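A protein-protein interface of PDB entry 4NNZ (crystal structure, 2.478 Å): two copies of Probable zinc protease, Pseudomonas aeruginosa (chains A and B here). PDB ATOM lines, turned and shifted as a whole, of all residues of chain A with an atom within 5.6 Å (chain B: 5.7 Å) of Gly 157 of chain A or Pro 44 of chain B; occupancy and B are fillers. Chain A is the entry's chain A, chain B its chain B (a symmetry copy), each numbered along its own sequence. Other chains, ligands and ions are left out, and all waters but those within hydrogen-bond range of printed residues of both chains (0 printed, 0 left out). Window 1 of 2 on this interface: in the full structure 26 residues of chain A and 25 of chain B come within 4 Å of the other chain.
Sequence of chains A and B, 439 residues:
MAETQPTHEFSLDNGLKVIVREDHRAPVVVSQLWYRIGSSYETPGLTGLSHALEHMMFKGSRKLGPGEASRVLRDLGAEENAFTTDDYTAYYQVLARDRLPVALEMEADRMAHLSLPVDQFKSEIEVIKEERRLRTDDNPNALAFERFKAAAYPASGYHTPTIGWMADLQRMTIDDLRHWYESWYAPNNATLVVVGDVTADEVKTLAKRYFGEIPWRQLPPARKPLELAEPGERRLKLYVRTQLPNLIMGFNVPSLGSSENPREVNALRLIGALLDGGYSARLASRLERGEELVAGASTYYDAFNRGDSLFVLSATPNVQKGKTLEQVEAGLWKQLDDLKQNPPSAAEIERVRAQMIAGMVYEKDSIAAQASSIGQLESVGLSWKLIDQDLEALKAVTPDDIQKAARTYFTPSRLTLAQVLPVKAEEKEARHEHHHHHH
OG1 of Thr 43 of chain A is in hydrogen-bond range of OG1 of Thr 43 of chain B.
The side-chain carboxylate (OD2) of Asp 168 of chain B sits close to the backbone NH (N) of Gly 45 of chain B.
O of Tyr 41 of chain A touches CG2 of Thr 43 of chain B, 3.7 Å away. Pro 44 of chain B touches Glu 42 of chain A. Glu 42 of chain B touches Pro 44 of chain A (O to CD, 3.7 Å). Pro 44 of chain B touches Gly 157 of chain A. Arg 223 of chain A touches Gly 45 of chain B.
Printed residues of chain A within 4 Å of Glu 42 of chain B: Pro 44. Printed residues of chain B within 4 Å of Pro 44 of chain A: Glu 42. Ser 40 of chain A touches none of the printed residues of chain B. Ser 39 of chain A touches none of the printed residues of chain B. The nearest printed residue of chain B that does not touch Gly 157 of chain A is Gly 45 of chain B (5.9 Å). The nearest printed residue of chain A that does not touch Gly 45 of chain B is Ala 155 of chain A (5.0 Å).
Of the 7 printed residues of chain B, 4 touch a printed residue of chain A. Of the 14 printed residues of chain A, 6 touch a printed residue of chain B. Among the printed residues, no Asp or Glu carboxylate lies within 4 Å of a Lys or Arg side-chain nitrogen of the other chain.
Glu 42 of chain A touches Pro 44 of chain B, and with the chains exchanged Pro 44 of chain A touches Glu 42 of chain B. Thr 43 of chain B touches its own counterpart, Thr 43 of chain A. Positions printed for both chains: 42, 43 and 44. Of the 6 pairs that touch across the chains among the printed residues, 3 have their exchanged pair printed and touching as well.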
ATOM      1  N   SER A  39      22.972 -12.511   9.333  1.00  0.00           N
ATOM      2  CA  SER A  39      23.394 -12.166   8.013  1.00  0.00           C
ATOM      3  C   SER A  39      24.047 -10.814   7.851  1.00  0.00           C
ATOM      4  O   SER A  39      24.756 -10.624   6.933  1.00  0.00           O
ATOM      5  CB  SER A  39      22.294 -12.394   6.994  1.00  0.00           C
ATOM      6  OG  SER A  39      21.126 -11.745   7.341  1.00  0.00           O
ATOM      7  N   SER A  40      23.788  -9.878   8.730  1.00  0.00           N
ATOM      8  CA  SER A  40      24.415  -8.582   8.642  1.00  0.00           C
ATOM      9  C   SER A  40      25.883  -8.618   9.031  1.00  0.00           C
ATOM     10  O   SER A  40      26.598  -7.706   8.785  1.00  0.00           O
ATOM     11  CB  SER A  40      23.635  -7.507   9.378  1.00  0.00           C
ATOM     12  OG  SER A  40      23.448  -7.793  10.725  1.00  0.00           O
ATOM     13  N   TYR A  41      26.321  -9.701   9.618  1.00  0.00           N
ATOM     14  CA  TYR A  41      27.702  -9.885   9.933  1.00  0.00           C
ATOM     15  C   TYR A  41      28.476 -10.490   8.789  1.00  0.00           C
ATOM     16  O   TYR A  41      29.664 -10.570   8.825  1.00  0.00           O
ATOM     17  CB  TYR A  41      27.812 -10.798  11.134  1.00  0.00           C
ATOM     18  CG  TYR A  41      27.252 -10.288  12.430  1.00  0.00           C
ATOM     19  CD1 TYR A  41      25.907 -10.208  12.644  1.00  0.00           C
ATOM     20  CD2 TYR A  41      28.076  -9.948  13.453  1.00  0.00           C
ATOM     21  CE1 TYR A  41      25.411  -9.775  13.831  1.00  0.00           C
ATOM     22  CE2 TYR A  41      27.580  -9.504  14.636  1.00  0.00           C
ATOM     23  CZ  TYR A  41      26.254  -9.422  14.818  1.00  0.00           C
ATOM     24  OH  TYR A  41      25.811  -8.993  16.004  1.00  0.00           O
ATOM     25  N   GLU A  42      27.766 -10.977   7.803  1.00  0.00           N
ATOM     26  CA  GLU A  42      28.343 -11.742   6.725  1.00  0.00           C
ATOM     27  C   GLU A  42      29.040 -10.919   5.677  1.00  0.00           C
ATOM     28  O   GLU A  42      28.837  -9.768   5.569  1.00  0.00           O
ATOM     29  CB  GLU A  42      27.299 -12.651   6.109  1.00  0.00           C
ATOM     30  CG  GLU A  42      26.951 -13.833   6.987  1.00  0.00           C
ATOM     31  CD  GLU A  42      25.662 -14.548   6.627  1.00  0.00           C
ATOM     32  OE1 GLU A  42      25.214 -14.508   5.485  1.00  0.00           O
ATOM     33  OE2 GLU A  42      25.099 -15.169   7.509  1.00  0.00           O
ATOM     34  N   THR A  43      29.865 -11.572   4.903  1.00  0.00           N
ATOM     35  CA  THR A  43      30.824 -10.946   4.039  1.00  0.00           C
ATOM     36  C   THR A  43      30.572 -11.428   2.656  1.00  0.00           C
ATOM     37  O   THR A  43      30.318 -12.575   2.481  1.00  0.00           O
ATOM     38  CB  THR A  43      32.231 -11.416   4.376  1.00  0.00           C
ATOM     39  OG1 THR A  43      32.520 -11.115   5.727  1.00  0.00           O
ATOM     40  CG2 THR A  43      33.207 -10.741   3.513  1.00  0.00           C
ATOM     41  N   PRO A  44      30.709 -10.593   1.654  1.00  0.00           N
ATOM     42  CA  PRO A  44      30.340 -10.999   0.311  1.00  0.00           C
ATOM     43  C   PRO A  44      31.144 -12.160  -0.194  1.00  0.00           C
ATOM     44  O   PRO A  44      32.319 -12.279   0.032  1.00  0.00           O
ATOM     45  CB  PRO A  44      30.626  -9.766  -0.505  1.00  0.00           C
ATOM     46  CG  PRO A  44      30.461  -8.666   0.439  1.00  0.00           C
ATOM     47  CD  PRO A  44      31.024  -9.168   1.712  1.00  0.00           C
ATOM     48  N   ALA A 155      24.976   0.730   2.198  1.00  0.00           N
ATOM     49  CA  ALA A 155      26.171   0.588   2.975  1.00  0.00           C
ATOM     50  C   ALA A 155      26.152  -0.432   4.079  1.00  0.00           C
ATOM     51  O   ALA A 155      27.188  -0.885   4.493  1.00  0.00           O
ATOM     52  CB  ALA A 155      26.568   1.927   3.532  1.00  0.00           C
ATOM     53  N   SER A 156      24.992  -0.760   4.601  1.00  0.00           N
ATOM     54  CA  SER A 156      24.919  -1.688   5.716  1.00  0.00           C
ATOM     55  C   SER A 156      24.794  -3.153   5.383  1.00  0.00           C
ATOM     56  O   SER A 156      24.526  -3.524   4.302  1.00  0.00           O
ATOM     57  CB  SER A 156      23.840  -1.275   6.702  1.00  0.00           C
ATOM     58  OG  SER A 156      22.562  -1.592   6.256  1.00  0.00           O
ATOM     59  N   GLY A 157      24.958  -3.972   6.383  1.00  0.00           N
ATOM     60  CA  GLY A 157      24.892  -5.395   6.226  1.00  0.00           C
ATOM     61  C   GLY A 157      23.496  -5.845   5.934  1.00  0.00           C
ATOM     62  O   GLY A 157      23.266  -6.950   5.557  1.00  0.00           O
ATOM     63  N   TYR A 158      22.562  -4.951   6.100  1.00  0.00           N
ATOM     64  CA  TYR A 158      21.193  -5.283   5.911  1.00  0.00           C
ATOM     65  C   TYR A 158      20.847  -5.628   4.528  1.00  0.00           C
ATOM     66  O   TYR A 158      19.840  -6.201   4.316  1.00  0.00           O
ATOM     67  CB  TYR A 158      20.279  -4.227   6.459  1.00  0.00           C
ATOM     68  CG  TYR A 158      20.209  -4.239   7.939  1.00  0.00           C
ATOM     69  CD1 TYR A 158      20.400  -5.394   8.645  1.00  0.00           C
ATOM     70  CD2 TYR A 158      19.972  -3.094   8.635  1.00  0.00           C
ATOM     71  CE1 TYR A 158      20.348  -5.399   9.988  1.00  0.00           C
ATOM     72  CE2 TYR A 158      19.924  -3.100   9.987  1.00  0.00           C
ATOM     73  CZ  TYR A 158      20.113  -4.261  10.643  1.00  0.00           C
ATOM     74  OH  TYR A 158      20.059  -4.306  11.969  1.00  0.00           O
ATOM     75  N   HIS A 159      21.667  -5.251   3.582  1.00  0.00           N
ATOM     76  CA  HIS A 159      21.367  -5.588   2.219  1.00  0.00           C
ATOM     77  C   HIS A 159      21.495  -7.034   1.914  1.00  0.00           C
ATOM     78  O   HIS A 159      20.934  -7.483   0.951  1.00  0.00           O
ATOM     79  CB  HIS A 159      22.058  -4.724   1.187  1.00  0.00           C
ATOM     80  CG  HIS A 159      23.534  -4.625   1.342  1.00  0.00           C
ATOM     81  ND1 HIS A 159      24.358  -5.717   1.375  1.00  0.00           N
ATOM     82  CD2 HIS A 159      24.342  -3.546   1.413  1.00  0.00           C
ATOM     83  CE1 HIS A 159      25.605  -5.318   1.498  1.00  0.00           C
ATOM     84  NE2 HIS A 159      25.624  -4.003   1.512  1.00  0.00           N
ATOM     85  N   THR A 160      22.209  -7.752   2.731  1.00  0.00           N
ATOM     86  CA  THR A 160      22.426  -9.125   2.399  1.00  0.00           C
ATOM     87  C   THR A 160      21.251 -10.028   2.704  1.00  0.00           C
ATOM     88  O   THR A 160      20.684  -9.955   3.751  1.00  0.00           O
ATOM     89  CB  THR A 160      23.806  -9.688   2.858  1.00  0.00           C
ATOM     90  OG1 THR A 160      23.635 -10.812   3.707  1.00  0.00           O
ATOM     91  CG2 THR A 160      24.649  -8.672   3.524  1.00  0.00           C
ATOM     92  N   ARG A 223      30.096  -4.518  14.185  1.00  0.00           N
ATOM     93  CA  ARG A 223      29.652  -3.162  14.048  1.00  0.00           C
ATOM     94  C   ARG A 223      28.186  -3.035  13.724  1.00  0.00           C
ATOM     95  O   ARG A 223      27.690  -3.753  12.926  1.00  0.00           O
ATOM     96  CB  ARG A 223      30.477  -2.496  12.970  1.00  0.00           C
ATOM     97  CG  ARG A 223      31.962  -2.672  13.127  1.00  0.00           C
ATOM     98  CD  ARG A 223      32.568  -1.468  13.786  1.00  0.00           C
ATOM     99  NE  ARG A 223      34.009  -1.500  13.771  1.00  0.00           N
ATOM    100  CZ  ARG A 223      34.731  -2.008  14.745  1.00  0.00           C
ATOM    101  NH1 ARG A 223      34.129  -2.524  15.775  1.00  0.00           N
ATOM    102  NH2 ARG A 223      36.032  -2.005  14.693  1.00  0.00           N
ATOM    103  N   PRO A 225      24.899  -2.100  11.996  1.00  0.00           N
ATOM    104  CA  PRO A 225      24.736  -1.835  10.582  1.00  0.00           C
ATOM    105  C   PRO A 225      24.079  -0.506  10.327  1.00  0.00           C
ATOM    106  O   PRO A 225      22.900  -0.422  10.163  1.00  0.00           O
ATOM    107  CB  PRO A 225      23.831  -2.957  10.121  1.00  0.00           C
ATOM    108  CG  PRO A 225      23.794  -3.922  11.207  1.00  0.00           C
ATOM    109  CD  PRO A 225      23.995  -3.154  12.438  1.00  0.00           C
ATOM    110  N   GLU B  42      36.064  -6.845   1.653  1.00  0.00           N
ATOM    111  CA  GLU B  42      35.731  -6.306   2.923  1.00  0.00           C
ATOM    112  C   GLU B  42      34.351  -6.593   3.431  1.00  0.00           C
ATOM    113  O   GLU B  42      33.421  -6.576   2.715  1.00  0.00           O
ATOM    114  CB  GLU B  42      36.001  -4.830   2.916  1.00  0.00           C
ATOM    115  CG  GLU B  42      37.433  -4.532   3.264  1.00  0.00           C
ATOM    116  CD  GLU B  42      37.921  -3.248   2.720  1.00  0.00           C
ATOM    117  OE1 GLU B  42      37.186  -2.279   2.735  1.00  0.00           O
ATOM    118  OE2 GLU B  42      39.046  -3.207   2.280  1.00  0.00           O
ATOM    119  N   THR B  43      34.275  -6.869   4.703  1.00  0.00           N
ATOM    120  CA  THR B  43      33.053  -7.022   5.439  1.00  0.00           C
ATOM    121  C   THR B  43      32.350  -5.733   5.728  1.00  0.00           C
ATOM    122  O   THR B  43      32.968  -4.760   5.990  1.00  0.00           O
ATOM    123  CB  THR B  43      33.357  -7.624   6.781  1.00  0.00           C
ATOM    124  OG1 THR B  43      34.337  -8.634   6.614  1.00  0.00           O
ATOM    125  CG2 THR B  43      32.153  -8.197   7.351  1.00  0.00           C
ATOM    126  N   PRO B  44      31.042  -5.750   5.763  1.00  0.00           N
ATOM    127  CA  PRO B  44      30.287  -4.557   6.103  1.00  0.00           C
ATOM    128  C   PRO B  44      30.528  -4.106   7.512  1.00  0.00           C
ATOM    129  O   PRO B  44      30.711  -4.885   8.400  1.00  0.00           O
ATOM    130  CB  PRO B  44      28.855  -4.995   5.948  1.00  0.00           C
ATOM    131  CG  PRO B  44      28.910  -6.093   5.008  1.00  0.00           C
ATOM    132  CD  PRO B  44      30.194  -6.789   5.196  1.00  0.00           C
ATOM    133  N   GLY B  45      30.573  -2.810   7.672  1.00  0.00           N
ATOM    134  CA  GLY B  45      30.935  -2.193   8.911  1.00  0.00           C
ATOM    135  C   GLY B  45      32.421  -2.109   9.055  1.00  0.00           C
ATOM    136  O   GLY B  45      32.887  -1.560   9.980  1.00  0.00           O
ATOM    137  N   LEU B  46      33.160  -2.706   8.150  1.00  0.00           N
ATOM    138  CA  LEU B  46      34.595  -2.683   8.204  1.00  0.00           C
ATOM    139  C   LEU B  46      35.202  -2.356   6.879  1.00  0.00           C
ATOM    140  O   LEU B  46      36.221  -2.853   6.530  1.00  0.00           O
ATOM    141  CB  LEU B  46      35.123  -3.995   8.723  1.00  0.00           C
ATOM    142  CG  LEU B  46      34.633  -4.316  10.115  1.00  0.00           C
ATOM    143  CD1 LEU B  46      34.081  -5.712  10.233  1.00  0.00           C
ATOM    144  CD2 LEU B  46      35.709  -4.061  11.128  1.00  0.00           C
ATOM    145  N   THR B  47      34.537  -1.520   6.131  1.00  0.00           N
ATOM    146  CA  THR B  47      35.064  -1.047   4.890  1.00  0.00           C
ATOM    147  C   THR B  47      36.181  -0.040   5.068  1.00  0.00           C
ATOM    148  O   THR B  47      36.257   0.639   6.048  1.00  0.00           O
ATOM    149  CB  THR B  47      33.949  -0.523   3.989  1.00  0.00           C
ATOM    150  OG1 THR B  47      33.364   0.622   4.559  1.00  0.00           O
ATOM    151  CG2 THR B  47      32.896  -1.517   3.887  1.00  0.00           C
ATOM    152  N   ASP B 168      32.069   3.355   8.857  1.00  0.00           N
ATOM    153  CA  ASP B 168      33.074   2.347   9.100  1.00  0.00           C
ATOM    154  C   ASP B 168      34.395   2.963   9.496  1.00  0.00           C
ATOM    155  O   ASP B 168      35.121   2.405  10.264  1.00  0.00           O
ATOM    156  CB  ASP B 168      33.267   1.409   7.926  1.00  0.00           C
ATOM    157  CG  ASP B 168      32.002   0.757   7.468  1.00  0.00           C
ATOM    158  OD1 ASP B 168      30.940   0.982   8.025  1.00  0.00           O
ATOM    159  OD2 ASP B 168      32.079   0.025   6.490  1.00  0.00           O
